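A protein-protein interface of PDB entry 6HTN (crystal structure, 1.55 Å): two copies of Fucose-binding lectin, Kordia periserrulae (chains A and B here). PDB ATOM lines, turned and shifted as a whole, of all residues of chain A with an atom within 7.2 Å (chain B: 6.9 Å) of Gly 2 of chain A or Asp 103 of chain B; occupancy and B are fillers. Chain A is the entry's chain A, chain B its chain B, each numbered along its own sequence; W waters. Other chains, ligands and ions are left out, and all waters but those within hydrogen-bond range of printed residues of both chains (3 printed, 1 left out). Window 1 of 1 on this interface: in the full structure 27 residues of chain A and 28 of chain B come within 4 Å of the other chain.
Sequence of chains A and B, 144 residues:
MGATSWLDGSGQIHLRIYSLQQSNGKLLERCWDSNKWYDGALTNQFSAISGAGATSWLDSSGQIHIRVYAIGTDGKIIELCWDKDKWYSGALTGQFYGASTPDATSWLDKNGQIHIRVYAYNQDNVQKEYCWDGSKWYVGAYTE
Water W2 lies within hydrogen-bond range of O of Ala 3 of chain A (2.6 Å) and O of Ala 104 of chain B (2.6 Å). Water W1 lies within hydrogen-bond range of the side-chain carboxylate (OD1) of Asp 103 of chain A (2.6 Å) and the backbone carbonyl oxygen (O) of Ala 52 of chain B (3.1 Å). Water W3 lies within hydrogen-bond range of the side-chain carboxylate of Asp 103 of chain B (2.7 Å), the backbone carbonyl oxygen of Ala 52 of chain A (3.1 Å) and the backbone NH of Gly 2 of chain A (3.4 Å).
Positions printed for both chains: 52, 53, 54, 101, 102 and 103.
Printed residues of chain A that touch a printed residue of chain B: Gly 2, Thr 4 and Ile 17. Hydrophobic or aromatic side chains of chain A within 4 Å of the printed part of chain B: Ile 17. Along chain A the printed residues that touch a printed residue of chain B span positions 2 to 17. Of the 14 printed residues of chain B, 3 touch a printed residue of chain A. Hydrophobic or aromatic side chains of chain B that line the printed part of chain A: Tyr 119. Among the printed residues, no Asp or Glu carboxylate lies within 4 Å of a Lys or Arg side-chain nitrogen of the other chain.
The side-chain carboxylate of Asp 103 of chain B sits at hydrogen-bond distance from the backbone NH of Gly 2 of chain A (2.7 Å).
Gly 2 of chain A touches just one residue of chain B: Asp 103. Printed residues of chain B within 4 Å of Thr 4 of chain A: Thr 105 (3.9 Å). Ala 52 of chain A touches none of the printed residues of chain B. Val 68 of chain A touches none of the printed residues of chain B. Printed residues of chain A within 4 Å of Asp 103 of chain B: Gly 2 (2.7 Å). Printed residues of chain A within 4 Å of Tyr 119 of chain B: Ile 17 (3.4 Å). The nearest residue of chain B that does not touch Gly 2 of chain A is Tyr 119 of chain B (6.1 Å). The nearest printed residue of chain A that does not touch Asp 103 of chain B is Ala 3 of chain A (4.02 Å). The nearest printed residue of chain A that does not touch Tyr 119 of chain B is Ala 3 of chain A (4.2 Å).
The backbone carbonyl oxygen of Ala 52 of chain A lies within hydrogen-bond range of the backbone NH of Gly 2 of chain A, at 2.7 Å. The backbone NH of Arg 117 of chain B sits at hydrogen-bond distance from the backbone carbonyl oxygen of Thr 105 of chain B, 2.9 Å away. The backbone carbonyl oxygen (O) of Asp 103 of chain B is in hydrogen-bond range of the backbone NH (N) of Tyr 119 of chain B. The backbone NH of Arg 16 of chain A sits at hydrogen-bond distance from the backbone carbonyl oxygen of Thr 4 of chain A, 2.9 Å away. The backbone carbonyl oxygen (O) of Gly 2 of chain A sits at hydrogen-bond distance from the backbone NH (N) of Tyr 18 of chain A, 2.8 Å away.
Among the printed residues, pairs that only touch across the chains: Ile 17 of chain A with Tyr 119 of chain B and Thr 4 of chain A with Thr 105 of chain B.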
ATOM      1  N   GLY A   2       2.054  20.450  18.157  1.00  0.00           N
ATOM      2  CA  GLY A   2       1.812  21.635  17.317  1.00  0.00           C
ATOM      3  C   GLY A   2       1.300  22.815  18.092  1.00  0.00           C
ATOM      4  O   GLY A   2       0.649  22.609  19.118  1.00  0.00           O
ATOM      5  N   ALA A   3       1.656  24.027  17.702  1.00  0.00           N
ATOM      6  CA  ALA A   3       1.214  25.268  18.358  1.00  0.00           C
ATOM      7  C   ALA A   3       0.687  26.221  17.315  1.00  0.00           C
ATOM      8  O   ALA A   3       1.396  26.429  16.283  1.00  0.00           O
ATOM      9  CB  ALA A   3       2.311  25.877  19.124  1.00  0.00           C
ATOM     10  N   THR A   4      -0.465  26.824  17.531  1.00  0.00           N
ATOM     11  CA  THR A   4      -0.954  27.884  16.624  1.00  0.00           C
ATOM     12  C   THR A   4      -1.565  28.969  17.481  1.00  0.00           C
ATOM     13  O   THR A   4      -1.905  28.699  18.663  1.00  0.00           O
ATOM     14  CB  THR A   4      -1.859  27.343  15.531  1.00  0.00           C
ATOM     15  OG1 THR A   4      -1.988  28.370  14.502  1.00  0.00           O
ATOM     16  CG2 THR A   4      -3.218  26.924  16.034  1.00  0.00           C
ATOM     17  N   ARG A  16      -3.597  27.590  20.794  1.00  0.00           N
ATOM     18  CA  ARG A  16      -4.101  26.211  20.670  1.00  0.00           C
ATOM     19  C   ARG A  16      -2.877  25.298  20.572  1.00  0.00           C
ATOM     20  O   ARG A  16      -2.095  25.466  19.596  1.00  0.00           O
ATOM     21  CB  ARG A  16      -5.079  25.990  19.542  1.00  0.00           C
ATOM     22  CG  ARG A  16      -6.338  26.843  19.640  1.00  0.00           C
ATOM     23  CD  ARG A  16      -7.240  26.322  20.778  1.00  0.00           C
ATOM     24  NE  ARG A  16      -8.509  27.105  20.830  1.00  0.00           N
ATOM     25  CZ  ARG A  16      -8.700  28.230  21.492  1.00  0.00           C
ATOM     26  NH1 ARG A  16      -7.754  28.843  22.129  1.00  0.00           N
ATOM     27  NH2 ARG A  16      -9.901  28.767  21.475  1.00  0.00           N
ATOM     28  N   ILE A  17      -2.711  24.389  21.514  1.00  0.00           N
ATOM     29  CA  ILE A  17      -1.509  23.519  21.621  1.00  0.00           C
ATOM     30  C   ILE A  17      -1.972  22.081  21.469  1.00  0.00           C
ATOM     31  O   ILE A  17      -2.805  21.615  22.294  1.00  0.00           O
ATOM     32  CB  ILE A  17      -0.757  23.778  22.924  1.00  0.00           C
ATOM     33  CG1 ILE A  17      -0.503  25.248  23.216  1.00  0.00           C
ATOM     34  CG2 ILE A  17       0.507  22.937  22.981  1.00  0.00           C
ATOM     35  CD1 ILE A  17       0.295  25.983  22.112  1.00  0.00           C
ATOM     36  N   TYR A  18      -1.435  21.343  20.519  1.00  0.00           N
ATOM     37  CA  TYR A  18      -1.847  19.982  20.164  1.00  0.00           C
ATOM     38  C   TYR A  18      -0.737  18.992  20.499  1.00  0.00           C
ATOM     39  O   TYR A  18       0.437  19.229  20.137  1.00  0.00           O
ATOM     40  CB  TYR A  18      -2.212  19.900  18.675  1.00  0.00           C
ATOM     41  CG  TYR A  18      -3.340  20.839  18.302  1.00  0.00           C
ATOM     42  CD1 TYR A  18      -4.674  20.468  18.501  1.00  0.00           C
ATOM     43  CD2 TYR A  18      -3.073  22.122  17.879  1.00  0.00           C
ATOM     44  CE1 TYR A  18      -5.701  21.373  18.245  1.00  0.00           C
ATOM     45  CE2 TYR A  18      -4.080  23.016  17.613  1.00  0.00           C
ATOM     46  CZ  TYR A  18      -5.400  22.645  17.800  1.00  0.00           C
ATOM     47  OH  TYR A  18      -6.404  23.597  17.639  1.00  0.00           O
ATOM     48  N   SER A  19      -1.110  17.899  21.131  1.00  0.00           N
ATOM     49  CA  SER A  19      -0.135  16.851  21.509  1.00  0.00           C
ATOM     50  C   SER A  19      -0.797  15.486  21.557  1.00  0.00           C
ATOM     51  O   SER A  19      -2.012  15.378  21.621  1.00  0.00           O
ATOM     52  CB  SER A  19       0.559  17.187  22.775  1.00  0.00           C
ATOM     53  OG  SER A  19      -0.374  17.222  23.895  1.00  0.00           O
ATOM     54  N   LEU A  20       0.008  14.430  21.472  1.00  0.00           N
ATOM     55  CA  LEU A  20      -0.460  13.027  21.473  1.00  0.00           C
ATOM     56  C   LEU A  20      -0.330  12.532  22.894  1.00  0.00           C
ATOM     57  O   LEU A  20       0.794  12.501  23.459  1.00  0.00           O
ATOM     58  CB  LEU A  20       0.376  12.188  20.509  1.00  0.00           C
ATOM     59  CG  LEU A  20       0.005  10.715  20.495  1.00  0.00           C
ATOM     60  CD1 LEU A  20      -1.416  10.505  20.029  1.00  0.00           C
ATOM     61  CD2 LEU A  20       0.990   9.978  19.619  1.00  0.00           C
ATOM     62  N   LEU A  28      -4.701  15.564  22.166  1.00  0.00           N
ATOM     63  CA  LEU A  28      -5.145  16.559  23.180  1.00  0.00           C
ATOM     64  C   LEU A  28      -5.049  17.931  22.544  1.00  0.00           C
ATOM     65  O   LEU A  28      -4.014  18.257  21.869  1.00  0.00           O
ATOM     66  CB  LEU A  28      -4.198  16.472  24.377  1.00  0.00           C
ATOM     67  CG  LEU A  28      -4.332  17.542  25.443  1.00  0.00           C
ATOM     68  CD1 LEU A  28      -5.702  17.476  26.098  1.00  0.00           C
ATOM     69  CD2 LEU A  28      -3.240  17.410  26.497  1.00  0.00           C
ATOM     70  N   GLY A  51       2.954  13.257  16.914  1.00  0.00           N
ATOM     71  CA  GLY A  51       2.487  14.599  17.267  1.00  0.00           C
ATOM     72  C   GLY A  51       1.745  15.215  16.114  1.00  0.00           C
ATOM     73  O   GLY A  51       1.541  14.619  15.063  1.00  0.00           O
ATOM     74  N   ALA A  52       1.329  16.456  16.294  1.00  0.00           N
ATOM     75  CA  ALA A  52       0.491  17.138  15.310  1.00  0.00           C
ATOM     76  C   ALA A  52       1.138  18.468  14.943  1.00  0.00           C
ATOM     77  O   ALA A  52       1.729  19.137  15.793  1.00  0.00           O
ATOM     78  CB  ALA A  52      -0.876  17.299  15.880  1.00  0.00           C
ATOM     79  N   GLY A  53       1.123  18.770  13.681  1.00  0.00           N
ATOM     80  CA  GLY A  53       1.427  20.122  13.202  1.00  0.00           C
ATOM     81  C   GLY A  53       0.123  20.875  13.056  1.00  0.00           C
ATOM     82  O   GLY A  53      -0.913  20.243  12.822  1.00  0.00           O
ATOM     83  N   ALA A  54       0.171  22.165  13.280  1.00  0.00           N
ATOM     84  CA  ALA A  54      -1.063  22.956  13.222  1.00  0.00           C
ATOM     85  C   ALA A  54      -0.833  24.260  12.476  1.00  0.00           C
ATOM     86  O   ALA A  54       0.250  24.883  12.635  1.00  0.00           O
ATOM     87  CB  ALA A  54      -1.544  23.196  14.632  1.00  0.00           C
ATOM     88  N   VAL A  68      -5.095  20.694  11.636  1.00  0.00           N
ATOM     89  CA  VAL A  68      -4.127  19.907  12.435  1.00  0.00           C
ATOM     90  C   VAL A  68      -3.803  18.659  11.627  1.00  0.00           C
ATOM     91  O   VAL A  68      -4.703  18.022  11.072  1.00  0.00           O
ATOM     92  CB  VAL A  68      -4.774  19.540  13.805  1.00  0.00           C
ATOM     93  CG1 VAL A  68      -3.925  18.669  14.631  1.00  0.00           C
ATOM     94  CG2 VAL A  68      -5.127  20.769  14.573  1.00  0.00           C
ATOM     95  N   THR A 101       6.224  13.638  12.126  1.00  0.00           N
ATOM     96  CA  THR A 101       5.201  14.581  12.596  1.00  0.00           C
ATOM     97  C   THR A 101       5.116  15.658  11.536  1.00  0.00           C
ATOM     98  O   THR A 101       6.099  16.357  11.321  1.00  0.00           O
ATOM     99  CB  THR A 101       5.508  15.176  13.957  1.00  0.00           C
ATOM    100  OG1 THR A 101       5.515  14.125  14.929  1.00  0.00           O
ATOM    101  CG2 THR A 101       4.504  16.237  14.341  1.00  0.00           C
ATOM    102  N   PRO A 102       3.955  15.857  10.889  1.00  0.00           N
ATOM    103  CA  PRO A 102       3.912  16.818   9.786  1.00  0.00           C
ATOM    104  C   PRO A 102       4.085  18.240  10.276  1.00  0.00           C
ATOM    105  O   PRO A 102       3.694  18.599  11.421  1.00  0.00           O
ATOM    106  CB  PRO A 102       2.509  16.648   9.211  1.00  0.00           C
ATOM    107  CG  PRO A 102       2.103  15.238   9.601  1.00  0.00           C
ATOM    108  CD  PRO A 102       2.739  15.025  10.930  1.00  0.00           C
ATOM    109  N   ASP A 103       4.691  19.049   9.414  1.00  0.00           N
ATOM    110  CA  ASP A 103       4.716  20.510   9.572  1.00  0.00           C
ATOM    111  C   ASP A 103       3.669  21.109   8.640  1.00  0.00           C
ATOM    112  O   ASP A 103       3.414  20.546   7.575  1.00  0.00           O
ATOM    113  CB  ASP A 103       6.077  21.089   9.164  1.00  0.00           C
ATOM    114  CG  ASP A 103       7.167  20.822  10.196  1.00  0.00           C
ATOM    115  OD1 ASP A 103       6.890  20.940  11.403  1.00  0.00           O
ATOM    116  OD2 ASP A 103       8.311  20.450   9.751  1.00  0.00           O
ATOM    117  N   ALA B  52      13.121  20.886  13.868  1.00  0.00           N
ATOM    118  CA  ALA B  52      13.102  22.275  14.338  1.00  0.00           C
ATOM    119  C   ALA B  52      11.665  22.796  14.269  1.00  0.00           C
ATOM    120  O   ALA B  52      10.886  22.400  13.375  1.00  0.00           O
ATOM    121  CB  ALA B  52      14.009  23.086  13.455  1.00  0.00           C
ATOM    122  N   GLY B  53      11.293  23.545  15.258  1.00  0.00           N
ATOM    123  CA  GLY B  53      10.085  24.359  15.202  1.00  0.00           C
ATOM    124  C   GLY B  53      10.412  25.741  14.758  1.00  0.00           C
ATOM    125  O   GLY B  53      11.502  26.167  15.046  1.00  0.00           O
ATOM    126  N   ALA B  54       9.500  26.400  14.083  1.00  0.00           N
ATOM    127  CA  ALA B  54       9.808  27.745  13.565  1.00  0.00           C
ATOM    128  C   ALA B  54       8.630  28.684  13.774  1.00  0.00           C
ATOM    129  O   ALA B  54       7.489  28.248  13.648  1.00  0.00           O
ATOM    130  CB  ALA B  54      10.186  27.685  12.108  1.00  0.00           C
ATOM    131  N   TYR B  69      13.766  26.630  16.677  1.00  0.00           N
ATOM    132  CA  TYR B  69      14.003  25.948  17.955  1.00  0.00           C
ATOM    133  C   TYR B  69      14.251  24.466  17.712  1.00  0.00           C
ATOM    134  O   TYR B  69      13.454  23.831  17.040  1.00  0.00           O
ATOM    135  CB  TYR B  69      12.835  26.181  18.904  1.00  0.00           C
ATOM    136  CG  TYR B  69      12.561  27.644  19.209  1.00  0.00           C
ATOM    137  CD1 TYR B  69      13.261  28.292  20.217  1.00  0.00           C
ATOM    138  CD2 TYR B  69      11.694  28.365  18.435  1.00  0.00           C
ATOM    139  CE1 TYR B  69      13.071  29.655  20.446  1.00  0.00           C
ATOM    140  CE2 TYR B  69      11.507  29.720  18.638  1.00  0.00           C
ATOM    141  CZ  TYR B  69      12.249  30.365  19.607  1.00  0.00           C
ATOM    142  OH  TYR B  69      12.061  31.716  19.833  1.00  0.00           O
ATOM    143  N   SER B 100      11.934  16.550  22.894  1.00  0.00           N
ATOM    144  CA  SER B 100      11.015  16.471  21.740  1.00  0.00           C
ATOM    145  C   SER B 100      11.332  17.629  20.795  1.00  0.00           C
ATOM    146  O   SER B 100      11.927  18.565  21.242  1.00  0.00           O
ATOM    147  CB  SER B 100       9.538  16.495  22.164  1.00  0.00           C
ATOM    148  OG  SER B 100       9.199  17.689  22.868  1.00  0.00           O
ATOM    149  N   THR B 101      10.938  17.536  19.530  1.00  0.00           N
ATOM    150  CA  THR B 101      11.096  18.639  18.561  1.00  0.00           C
ATOM    151  C   THR B 101      10.241  19.778  19.078  1.00  0.00           C
ATOM    152  O   THR B 101       9.021  19.615  19.163  1.00  0.00           O
ATOM    153  CB  THR B 101      10.674  18.209  17.161  1.00  0.00           C
ATOM    154  OG1 THR B 101      11.587  17.179  16.751  1.00  0.00           O
ATOM    155  CG2 THR B 101      10.695  19.382  16.206  1.00  0.00           C
ATOM    156  N   PRO B 102      10.822  20.951  19.410  1.00  0.00           N
ATOM    157  CA  PRO B 102      10.020  22.032  19.917  1.00  0.00           C
ATOM    158  C   PRO B 102       8.975  22.571  18.952  1.00  0.00           C
ATOM    159  O   PRO B 102       9.167  22.563  17.723  1.00  0.00           O
ATOM    160  CB  PRO B 102      11.018  23.140  20.267  1.00  0.00           C
ATOM    161  CG  PRO B 102      12.316  22.390  20.434  1.00  0.00           C
ATOM    162  CD  PRO B 102      12.238  21.269  19.424  1.00  0.00           C
ATOM    163  N   ASP B 103       7.841  22.973  19.529  1.00  0.00           N
ATOM    164  CA  ASP B 103       6.826  23.759  18.820  1.00  0.00           C
ATOM    165  C   ASP B 103       6.977  25.216  19.233  1.00  0.00           C
ATOM    166  O   ASP B 103       7.398  25.494  20.361  1.00  0.00           O
ATOM    167  CB  ASP B 103       5.435  23.282  19.255  1.00  0.00           C
ATOM    168  CG  ASP B 103       5.004  21.997  18.606  1.00  0.00           C
ATOM    169  OD1 ASP B 103       5.258  21.831  17.401  1.00  0.00           O
ATOM    170  OD2 ASP B 103       4.377  21.180  19.282  1.00  0.00           O
ATOM    171  N   ALA B 104       6.622  26.122  18.355  1.00  0.00           N
ATOM    172  CA  ALA B 104       6.712  27.572  18.693  1.00  0.00           C
ATOM    173  C   ALA B 104       5.593  28.328  18.002  1.00  0.00           C
ATOM    174  O   ALA B 104       5.187  27.997  16.909  1.00  0.00           O
ATOM    175  CB  ALA B 104       8.044  28.151  18.315  1.00  0.00           C
ATOM    176  N   THR B 105       5.102  29.366  18.667  1.00  0.00           N
ATOM    177  CA  THR B 105       4.185  30.349  18.065  1.00  0.00           C
ATOM    178  C   THR B 105       4.565  31.724  18.610  1.00  0.00           C
ATOM    179  O   THR B 105       5.284  31.828  19.601  1.00  0.00           O
ATOM    180  CB  THR B 105       2.727  29.961  18.267  1.00  0.00           C
ATOM    181  OG1 THR B 105       1.863  30.723  17.429  1.00  0.00           O
ATOM    182  CG2 THR B 105       2.296  30.080  19.715  1.00  0.00           C
ATOM    183  N   ARG B 117       6.060  31.789  22.399  1.00  0.00           N
ATOM    184  CA  ARG B 117       5.819  30.649  23.287  1.00  0.00           C
ATOM    185  C   ARG B 117       6.405  29.403  22.607  1.00  0.00           C
ATOM    186  O   ARG B 117       6.105  29.159  21.416  1.00  0.00           O
ATOM    187  CB  ARG B 117       4.346  30.457  23.581  1.00  0.00           C
ATOM    188  CG  ARG B 117       3.647  31.671  24.209  1.00  0.00           C
ATOM    189  CD  ARG B 117       4.138  31.853  25.632  1.00  0.00           C
ATOM    190  NE  ARG B 117       3.479  32.962  26.364  1.00  0.00           N
ATOM    191  CZ  ARG B 117       3.931  34.197  26.381  1.00  0.00           C
ATOM    192  NH1 ARG B 117       5.005  34.574  25.704  1.00  0.00           N
ATOM    193  NH2 ARG B 117       3.273  35.107  27.098  1.00  0.00           N
ATOM    194  N   VAL B 118       7.262  28.707  23.314  1.00  0.00           N
ATOM    195  CA  VAL B 118       7.965  27.487  22.838  1.00  0.00           C
ATOM    196  C   VAL B 118       7.535  26.328  23.728  1.00  0.00           C
ATOM    197  O   VAL B 118       7.516  26.487  24.948  1.00  0.00           O
ATOM    198  CB  VAL B 118       9.465  27.713  22.925  1.00  0.00           C
ATOM    199  CG1 VAL B 118      10.245  26.448  22.520  1.00  0.00           C
ATOM    200  CG2 VAL B 118       9.877  28.890  22.045  1.00  0.00           C
ATOM    201  N   TYR B 119       7.234  25.181  23.129  1.00  0.00           N
ATOM    202  CA  TYR B 119       6.739  24.011  23.894  1.00  0.00           C
ATOM    203  C   TYR B 119       7.640  22.815  23.594  1.00  0.00           C
ATOM    204  O   TYR B 119       7.957  22.568  22.437  1.00  0.00           O
ATOM    205  CB  TYR B 119       5.305  23.719  23.494  1.00  0.00           C
ATOM    206  CG  TYR B 119       4.361  24.877  23.705  1.00  0.00           C
ATOM    207  CD1 TYR B 119       4.269  25.885  22.790  1.00  0.00           C
ATOM    208  CD2 TYR B 119       3.614  24.975  24.880  1.00  0.00           C
ATOM    209  CE1 TYR B 119       3.471  27.010  23.022  1.00  0.00           C
ATOM    210  CE2 TYR B 119       2.785  26.057  25.112  1.00  0.00           C
ATOM    211  CZ  TYR B 119       2.748  27.087  24.189  1.00  0.00           C
ATOM    212  OH  TYR B 119       1.977  28.209  24.393  1.00  0.00           O
ATOM    213  N   ALA B 120       8.035  22.099  24.638  1.00  0.00           N
ATOM    214  CA  ALA B 120       8.831  20.875  24.456  1.00  0.00           C
ATOM    215  C   ALA B 120       8.764  20.040  25.722  1.00  0.00           C
ATOM    216  O   ALA B 120       8.747  20.600  26.826  1.00  0.00           O
ATOM    217  CB  ALA B 120      10.260  21.157  24.119  1.00  0.00           C
HETATM  218  O   HOH W   1       8.672  20.280  13.235  1.00  0.00           O
HETATM  219  O   HOH W   2       3.540  27.114  15.066  1.00  0.00           O
HETATM  220  O   HOH W   3       4.756  19.420  16.337  1.00  0.00           O
